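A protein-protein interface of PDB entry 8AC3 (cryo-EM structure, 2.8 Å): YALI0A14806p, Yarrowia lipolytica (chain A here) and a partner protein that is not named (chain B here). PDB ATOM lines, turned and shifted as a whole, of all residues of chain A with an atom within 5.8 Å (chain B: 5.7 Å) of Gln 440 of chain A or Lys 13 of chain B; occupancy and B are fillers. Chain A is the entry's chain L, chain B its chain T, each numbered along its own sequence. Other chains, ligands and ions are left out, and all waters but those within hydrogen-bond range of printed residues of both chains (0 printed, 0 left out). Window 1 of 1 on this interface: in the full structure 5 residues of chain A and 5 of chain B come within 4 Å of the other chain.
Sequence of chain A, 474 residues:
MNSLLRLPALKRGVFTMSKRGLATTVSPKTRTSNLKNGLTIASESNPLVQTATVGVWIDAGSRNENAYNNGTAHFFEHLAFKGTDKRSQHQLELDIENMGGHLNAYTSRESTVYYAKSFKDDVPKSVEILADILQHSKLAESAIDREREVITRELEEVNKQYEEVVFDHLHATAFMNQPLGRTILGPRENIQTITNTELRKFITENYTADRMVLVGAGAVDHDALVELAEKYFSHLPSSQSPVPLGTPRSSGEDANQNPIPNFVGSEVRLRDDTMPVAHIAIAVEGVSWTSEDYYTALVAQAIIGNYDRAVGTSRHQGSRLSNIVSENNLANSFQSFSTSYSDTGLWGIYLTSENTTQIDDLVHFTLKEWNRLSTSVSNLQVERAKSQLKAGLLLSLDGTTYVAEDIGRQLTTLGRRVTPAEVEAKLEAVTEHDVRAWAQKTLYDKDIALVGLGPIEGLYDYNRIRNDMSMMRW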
ATOM      1  N   LEU A 373      17.746  -9.257  28.148  1.00  0.00           N
ATOM      2  CA  LEU A 373      16.658  -8.548  28.803  1.00  0.00           C
ATOM      3  C   LEU A 373      15.601  -8.189  27.776  1.00  0.00           C
ATOM      4  O   LEU A 373      14.442  -8.016  28.137  1.00  0.00           O
ATOM      5  CB  LEU A 373      17.164  -7.280  29.483  1.00  0.00           C
ATOM      6  CG  LEU A 373      18.054  -7.515  30.695  1.00  0.00           C
ATOM      7  CD1 LEU A 373      18.691  -6.215  31.146  1.00  0.00           C
ATOM      8  CD2 LEU A 373      17.224  -8.083  31.820  1.00  0.00           C
ATOM      9  N   SER A 374      16.026  -8.049  26.513  1.00  0.00           N
ATOM     10  CA  SER A 374      15.134  -7.699  25.422  1.00  0.00           C
ATOM     11  C   SER A 374      14.530  -8.954  24.818  1.00  0.00           C
ATOM     12  O   SER A 374      13.384  -8.922  24.390  1.00  0.00           O
ATOM     13  CB  SER A 374      15.818  -6.904  24.343  1.00  0.00           C
ATOM     14  OG  SER A 374      16.164  -5.617  24.814  1.00  0.00           O
ATOM     15  N   THR A 375      15.293 -10.044  24.772  1.00  0.00           N
ATOM     16  CA  THR A 375      14.873 -11.106  23.880  1.00  0.00           C
ATOM     17  C   THR A 375      14.304 -12.282  24.652  1.00  0.00           C
ATOM     18  O   THR A 375      13.452 -12.980  24.113  1.00  0.00           O
ATOM     19  CB  THR A 375      16.026 -11.619  23.018  1.00  0.00           C
ATOM     20  OG1 THR A 375      16.943 -12.294  23.880  1.00  0.00           O
ATOM     21  CG2 THR A 375      16.708 -10.511  22.248  1.00  0.00           C
ATOM     22  N   VAL A 435       9.546  -5.622  31.728  1.00  0.00           N
ATOM     23  CA  VAL A 435      10.988  -5.592  31.599  1.00  0.00           C
ATOM     24  C   VAL A 435      11.395  -5.700  30.136  1.00  0.00           C
ATOM     25  O   VAL A 435      12.211  -4.896  29.686  1.00  0.00           O
ATOM     26  CB  VAL A 435      11.667  -6.660  32.457  1.00  0.00           C
ATOM     27  CG1 VAL A 435      13.167  -6.717  32.199  1.00  0.00           C
ATOM     28  CG2 VAL A 435      11.383  -6.398  33.921  1.00  0.00           C
ATOM     29  N   ARG A 436      10.830  -6.664  29.399  1.00  0.00           N
ATOM     30  CA  ARG A 436      11.177  -6.773  27.987  1.00  0.00           C
ATOM     31  C   ARG A 436      10.875  -5.463  27.253  1.00  0.00           C
ATOM     32  O   ARG A 436      11.676  -5.014  26.437  1.00  0.00           O
ATOM     33  CB  ARG A 436      10.439  -7.901  27.257  1.00  0.00           C
ATOM     34  CG  ARG A 436      10.860  -9.324  27.600  1.00  0.00           C
ATOM     35  CD  ARG A 436       9.722 -10.298  27.294  1.00  0.00           C
ATOM     36  NE  ARG A 436       9.701 -10.398  25.849  1.00  0.00           N
ATOM     37  CZ  ARG A 436      10.634 -11.048  25.174  1.00  0.00           C
ATOM     38  NH1 ARG A 436      11.603 -11.663  25.831  1.00  0.00           N
ATOM     39  NH2 ARG A 436      10.601 -11.085  23.857  1.00  0.00           N
ATOM     40  N   ALA A 437       9.715  -4.857  27.526  1.00  0.00           N
ATOM     41  CA  ALA A 437       9.369  -3.632  26.822  1.00  0.00           C
ATOM     42  C   ALA A 437      10.403  -2.551  27.105  1.00  0.00           C
ATOM     43  O   ALA A 437      10.758  -1.796  26.204  1.00  0.00           O
ATOM     44  CB  ALA A 437       8.011  -3.142  27.233  1.00  0.00           C
ATOM     45  N   TRP A 438      10.811  -2.451  28.373  1.00  0.00           N
ATOM     46  CA  TRP A 438      11.683  -1.373  28.779  1.00  0.00           C
ATOM     47  C   TRP A 438      13.044  -1.583  28.143  1.00  0.00           C
ATOM     48  O   TRP A 438      13.624  -0.634  27.634  1.00  0.00           O
ATOM     49  CB  TRP A 438      11.767  -1.263  30.301  1.00  0.00           C
ATOM     50  CG  TRP A 438      12.805  -0.291  30.762  1.00  0.00           C
ATOM     51  CD1 TRP A 438      12.655   1.052  30.957  1.00  0.00           C
ATOM     52  CD2 TRP A 438      14.164  -0.602  31.113  1.00  0.00           C
ATOM     53  NE1 TRP A 438      13.843   1.595  31.373  1.00  0.00           N
ATOM     54  CE2 TRP A 438      14.777   0.602  31.512  1.00  0.00           C
ATOM     55  CE3 TRP A 438      14.917  -1.784  31.139  1.00  0.00           C
ATOM     56  CZ2 TRP A 438      16.119   0.654  31.898  1.00  0.00           C
ATOM     57  CZ3 TRP A 438      16.239  -1.734  31.524  1.00  0.00           C
ATOM     58  CH2 TRP A 438      16.832  -0.527  31.891  1.00  0.00           C
ATOM     59  N   ALA A 439      13.514  -2.832  28.151  1.00  0.00           N
ATOM     60  CA  ALA A 439      14.855  -3.116  27.663  1.00  0.00           C
ATOM     61  C   ALA A 439      14.926  -2.865  26.161  1.00  0.00           C
ATOM     62  O   ALA A 439      15.943  -2.408  25.637  1.00  0.00           O
ATOM     63  CB  ALA A 439      15.223  -4.530  28.005  1.00  0.00           C
ATOM     64  N   GLN A 440      13.817  -3.138  25.475  1.00  0.00           N
ATOM     65  CA  GLN A 440      13.803  -3.012  24.031  1.00  0.00           C
ATOM     66  C   GLN A 440      13.796  -1.550  23.621  1.00  0.00           C
ATOM     67  O   GLN A 440      14.199  -1.226  22.513  1.00  0.00           O
ATOM     68  CB  GLN A 440      12.592  -3.708  23.445  1.00  0.00           C
ATOM     69  CG  GLN A 440      12.869  -5.174  23.228  1.00  0.00           C
ATOM     70  CD  GLN A 440      11.578  -5.890  22.962  1.00  0.00           C
ATOM     71  OE1 GLN A 440      10.567  -5.287  22.616  1.00  0.00           O
ATOM     72  NE2 GLN A 440      11.601  -7.193  23.147  1.00  0.00           N
ATOM     73  N   LYS A 441      13.363  -0.671  24.525  1.00  0.00           N
ATOM     74  CA  LYS A 441      13.301   0.751  24.235  1.00  0.00           C
ATOM     75  C   LYS A 441      14.559   1.468  24.745  1.00  0.00           C
ATOM     76  O   LYS A 441      14.914   2.525  24.229  1.00  0.00           O
ATOM     77  CB  LYS A 441      11.910   1.197  24.694  1.00  0.00           C
ATOM     78  CG  LYS A 441      11.732   2.453  25.527  1.00  0.00           C
ATOM     79  CD  LYS A 441      10.270   2.707  25.737  1.00  0.00           C
ATOM     80  CE  LYS A 441       9.930   3.138  27.148  1.00  0.00           C
ATOM     81  NZ  LYS A 441      10.315   4.548  27.413  1.00  0.00           N
ATOM     82  N   THR A 442      15.269   0.862  25.704  1.00  0.00           N
ATOM     83  CA  THR A 442      16.278   1.574  26.469  1.00  0.00           C
ATOM     84  C   THR A 442      17.660   0.989  26.241  1.00  0.00           C
ATOM     85  O   THR A 442      18.645   1.713  26.281  1.00  0.00           O
ATOM     86  CB  THR A 442      15.961   1.504  27.962  1.00  0.00           C
ATOM     87  OG1 THR A 442      14.674   2.096  28.112  1.00  0.00           O
ATOM     88  CG2 THR A 442      16.965   2.234  28.824  1.00  0.00           C
ATOM     89  N   LEU A 443      17.723  -0.313  25.990  1.00  0.00           N
ATOM     90  CA  LEU A 443      19.016  -0.946  25.862  1.00  0.00           C
ATOM     91  C   LEU A 443      19.253  -1.424  24.446  1.00  0.00           C
ATOM     92  O   LEU A 443      20.370  -1.321  23.958  1.00  0.00           O
ATOM     93  CB  LEU A 443      19.032  -2.171  26.754  1.00  0.00           C
ATOM     94  CG  LEU A 443      19.338  -1.879  28.203  1.00  0.00           C
ATOM     95  CD1 LEU A 443      19.001  -3.127  28.985  1.00  0.00           C
ATOM     96  CD2 LEU A 443      20.816  -1.548  28.315  1.00  0.00           C
ATOM     97  N   TYR A 444      18.227  -2.021  23.836  1.00  0.00           N
ATOM     98  CA  TYR A 444      18.461  -2.795  22.634  1.00  0.00           C
ATOM     99  C   TYR A 444      18.931  -1.866  21.531  1.00  0.00           C
ATOM    100  O   TYR A 444      18.231  -0.906  21.222  1.00  0.00           O
ATOM    101  CB  TYR A 444      17.198  -3.504  22.157  1.00  0.00           C
ATOM    102  CG  TYR A 444      17.564  -4.596  21.195  1.00  0.00           C
ATOM    103  CD1 TYR A 444      18.189  -5.737  21.672  1.00  0.00           C
ATOM    104  CD2 TYR A 444      17.395  -4.460  19.822  1.00  0.00           C
ATOM    105  CE1 TYR A 444      18.588  -6.755  20.826  1.00  0.00           C
ATOM    106  CE2 TYR A 444      17.796  -5.470  18.957  1.00  0.00           C
ATOM    107  CZ  TYR A 444      18.397  -6.618  19.463  1.00  0.00           C
ATOM    108  OH  TYR A 444      18.807  -7.632  18.644  1.00  0.00           O
ATOM    109  N   LYS A 446      21.131   0.483  21.407  1.00  0.00           N
ATOM    110  CA  LYS A 446      21.201   1.891  21.763  1.00  0.00           C
ATOM    111  C   LYS A 446      22.657   2.278  21.934  1.00  0.00           C
ATOM    112  O   LYS A 446      23.501   1.405  22.045  1.00  0.00           O
ATOM    113  CB  LYS A 446      20.458   2.167  23.065  1.00  0.00           C
ATOM    114  CG  LYS A 446      18.952   2.018  22.968  1.00  0.00           C
ATOM    115  CD  LYS A 446      18.333   3.148  22.180  1.00  0.00           C
ATOM    116  CE  LYS A 446      17.895   4.285  23.077  1.00  0.00           C
ATOM    117  NZ  LYS A 446      17.915   5.584  22.362  1.00  0.00           N
ATOM    118  N   TRP A 474      18.338 -12.454  16.480  1.00  0.00           N
ATOM    119  CA  TRP A 474      17.006 -12.091  16.916  1.00  0.00           C
ATOM    120  C   TRP A 474      16.426 -11.047  15.967  1.00  0.00           C
ATOM    121  O   TRP A 474      15.481 -11.423  15.263  1.00  0.00           O
ATOM    122  CB  TRP A 474      17.047 -11.554  18.337  1.00  0.00           C
ATOM    123  CG  TRP A 474      15.718 -11.252  18.959  1.00  0.00           C
ATOM    124  CD1 TRP A 474      14.851 -12.149  19.508  1.00  0.00           C
ATOM    125  CD2 TRP A 474      15.163  -9.953  19.228  1.00  0.00           C
ATOM    126  NE1 TRP A 474      13.786 -11.501  20.068  1.00  0.00           N
ATOM    127  CE2 TRP A 474      13.938 -10.154  19.895  1.00  0.00           C
ATOM    128  CE3 TRP A 474      15.566  -8.646  18.952  1.00  0.00           C
ATOM    129  CZ2 TRP A 474      13.118  -9.097  20.285  1.00  0.00           C
ATOM    130  CZ3 TRP A 474      14.764  -7.594  19.343  1.00  0.00           C
ATOM    131  CH2 TRP A 474      13.552  -7.820  20.004  1.00  0.00           C
ATOM    132  N   TYR B   8      10.446   1.746  13.067  1.00  0.00           N
ATOM    133  CA  TYR B   8      11.649   1.121  13.590  1.00  0.00           C
ATOM    134  C   TYR B   8      11.327  -0.208  14.273  1.00  0.00           C
ATOM    135  O   TYR B   8      11.963  -1.225  13.993  1.00  0.00           O
ATOM    136  CB  TYR B   8      12.416   2.046  14.536  1.00  0.00           C
ATOM    137  CG  TYR B   8      13.566   1.322  15.180  1.00  0.00           C
ATOM    138  CD1 TYR B   8      14.768   1.156  14.502  1.00  0.00           C
ATOM    139  CD2 TYR B   8      13.428   0.735  16.431  1.00  0.00           C
ATOM    140  CE1 TYR B   8      15.815   0.436  15.052  1.00  0.00           C
ATOM    141  CE2 TYR B   8      14.471   0.018  16.999  1.00  0.00           C
ATOM    142  CZ  TYR B   8      15.669  -0.129  16.308  1.00  0.00           C
ATOM    143  OH  TYR B   8      16.719  -0.823  16.842  1.00  0.00           O
ATOM    144  N   ASN B   9      10.351  -0.170  15.185  1.00  0.00           N
ATOM    145  CA  ASN B   9       9.997  -1.311  16.017  1.00  0.00           C
ATOM    146  C   ASN B   9       9.517  -2.499  15.194  1.00  0.00           C
ATOM    147  O   ASN B   9       9.816  -3.641  15.534  1.00  0.00           O
ATOM    148  CB  ASN B   9       8.920  -0.972  17.039  1.00  0.00           C
ATOM    149  CG  ASN B   9       9.514  -0.236  18.212  1.00  0.00           C
ATOM    150  OD1 ASN B   9      10.665  -0.471  18.570  1.00  0.00           O
ATOM    151  ND2 ASN B   9       8.749   0.675  18.790  1.00  0.00           N
ATOM    152  N   VAL B  10       8.791  -2.232  14.108  1.00  0.00           N
ATOM    153  CA  VAL B  10       8.229  -3.296  13.298  1.00  0.00           C
ATOM    154  C   VAL B  10       9.266  -3.873  12.337  1.00  0.00           C
ATOM    155  O   VAL B  10       9.411  -5.091  12.277  1.00  0.00           O
ATOM    156  CB  VAL B  10       6.961  -2.830  12.572  1.00  0.00           C
ATOM    157  CG1 VAL B  10       6.430  -3.911  11.651  1.00  0.00           C
ATOM    158  CG2 VAL B  10       5.902  -2.460  13.589  1.00  0.00           C
ATOM    159  N   PHE B  11       9.997  -3.027  11.607  1.00  0.00           N
ATOM    160  CA  PHE B  11      10.737  -3.576  10.486  1.00  0.00           C
ATOM    161  C   PHE B  11      12.222  -3.692  10.770  1.00  0.00           C
ATOM    162  O   PHE B  11      12.927  -4.373  10.029  1.00  0.00           O
ATOM    163  CB  PHE B  11      10.513  -2.740   9.235  1.00  0.00           C
ATOM    164  CG  PHE B  11       9.079  -2.775   8.783  1.00  0.00           C
ATOM    165  CD1 PHE B  11       8.568  -3.889   8.137  1.00  0.00           C
ATOM    166  CD2 PHE B  11       8.230  -1.708   9.038  1.00  0.00           C
ATOM    167  CE1 PHE B  11       7.243  -3.926   7.727  1.00  0.00           C
ATOM    168  CE2 PHE B  11       6.903  -1.747   8.636  1.00  0.00           C
ATOM    169  CZ  PHE B  11       6.414  -2.853   7.975  1.00  0.00           C
ATOM    170  N   VAL B  12      12.700  -3.018  11.817  1.00  0.00           N
ATOM    171  CA  VAL B  12      14.137  -2.855  11.921  1.00  0.00           C
ATOM    172  C   VAL B  12      14.673  -3.483  13.199  1.00  0.00           C
ATOM    173  O   VAL B  12      15.722  -4.112  13.171  1.00  0.00           O
ATOM    174  CB  VAL B  12      14.535  -1.380  11.759  1.00  0.00           C
ATOM    175  CG1 VAL B  12      16.036  -1.210  11.828  1.00  0.00           C
ATOM    176  CG2 VAL B  12      14.034  -0.869  10.429  1.00  0.00           C
ATOM    177  N   LYS B  13      13.952  -3.330  14.307  1.00  0.00           N
ATOM    178  CA  LYS B  13      14.470  -3.712  15.613  1.00  0.00           C
ATOM    179  C   LYS B  13      14.910  -5.178  15.645  1.00  0.00           C
ATOM    180  O   LYS B  13      16.017  -5.470  16.079  1.00  0.00           O
ATOM    181  CB  LYS B  13      13.438  -3.393  16.693  1.00  0.00           C
ATOM    182  CG  LYS B  13      13.772  -3.859  18.102  1.00  0.00           C
ATOM    183  CD  LYS B  13      12.803  -3.331  19.165  1.00  0.00           C
ATOM    184  CE  LYS B  13      11.471  -4.056  19.212  1.00  0.00           C
ATOM    185  NZ  LYS B  13      10.463  -3.368  20.060  1.00  0.00           N
ATOM    186  N   ARG B  14      14.040  -6.097  15.217  1.00  0.00           N
ATOM    187  CA  ARG B  14      14.404  -7.503  15.155  1.00  0.00           C
ATOM    188  C   ARG B  14      15.133  -7.757  13.843  1.00  0.00           C
ATOM    189  O   ARG B  14      14.642  -7.367  12.792  1.00  0.00           O
ATOM    190  CB  ARG B  14      13.152  -8.374  15.196  1.00  0.00           C
ATOM    191  CG  ARG B  14      12.538  -8.468  16.580  1.00  0.00           C
ATOM    192  CD  ARG B  14      11.094  -8.905  16.484  1.00  0.00           C
ATOM    193  NE  ARG B  14      10.368  -8.641  17.716  1.00  0.00           N
ATOM    194  CZ  ARG B  14       9.788  -7.483  18.014  1.00  0.00           C
ATOM    195  NH1 ARG B  14       9.843  -6.464  17.172  1.00  0.00           N
ATOM    196  NH2 ARG B  14       9.153  -7.344  19.162  1.00  0.00           N
ATOM    197  N   ASN B  15      16.308  -8.390  13.907  1.00  0.00           N
ATOM    198  CA  ASN B  15      17.062  -8.673  12.701  1.00  0.00           C
ATOM    199  C   ASN B  15      16.301  -9.649  11.812  1.00  0.00           C
ATOM    200  O   ASN B  15      16.352  -9.548  10.590  1.00  0.00           O
ATOM    201  CB  ASN B  15      18.451  -9.232  12.996  1.00  0.00           C
ATOM    202  CG  ASN B  15      19.368  -9.099  11.804  1.00  0.00           C
ATOM    203  OD1 ASN B  15      19.414  -8.027  11.202  1.00  0.00           O
ATOM    204  ND2 ASN B  15      20.101 -10.153  11.467  1.00  0.00           N
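The backbone carbonyl oxygen of Ser 374 of chain A sits at hydrogen-bond distance from the side-chain amide nitrogen of Gln 440 of chain A, 2.8 Å away. The backbone carbonyl oxygen of Ala 439 of chain A lies within hydrogen-bond range of the backbone NH of Tyr 444 of chain A (2.9 Å). O of Tyr 8 of chain B is in hydrogen-bond range of N of Lys 13 of chain B. The side-chain amino group of Lys 13 of chain B is in hydrogen-bond range of the side-chain amide oxygen of Asn 9 of chain B (3.3 Å). NH1 of Arg 14 of chain B lies within hydrogen-bond range of O of Asn 9 of chain B (3.3 Å).
O of Lys 13 of chain B touches CE2 of Tyr 444 of chain A, 3.4 Å away. Arg 14 of chain B touches Trp 474 of chain A.
Printed residues of chain B within 4 Å of Gln 440 of chain A: Lys 13. Lys 441 of chain A touches none of the printed residues of chain B. Printed residues of chain B within 4 Å of Tyr 444 of chain A: Lys 13 (3.4 Å). Printed residues of chain B within 4 Å of Trp 474 of chain A: Arg 14 and Asn 15. Phe 11 of chain B touches none of the printed residues of chain A. Lys 13 of chain B touches two residues of chain A. Of the printed residues of chain A, Arg 14 of chain B touches Trp 474 (3.6 Å). Of the printed residues of chain A, Asn 15 of chain B touches Trp 474. The nearest residue of chain A that does not touch Lys 13 of chain B is Trp 474 of chain A (4.1 Å).
The side-chain amide oxygen (OE1) of Gln 440 of chain A lies within hydrogen-bond range of the side-chain amino group (NZ) of Lys 13 of chain B (3.2 Å). The backbone carbonyl oxygen (O) of Trp 474 of chain A lies close to the backbone NH (N) of Asn 15 of chain B, at 3.4 Å.
Of the 8 printed residues of chain B, 3 touch a printed residue of chain A. Along chain B the printed residues that touch a printed residue of chain A span positions 13 to 15. Hydrophobic or aromatic side chains of chain A that line the printed part of chain B: Tyr 444 and Trp 474. Among the printed residues, no Asp or Glu carboxylate lies within 4 Å of a Lys or Arg side-chain nitrogen of the other chain.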
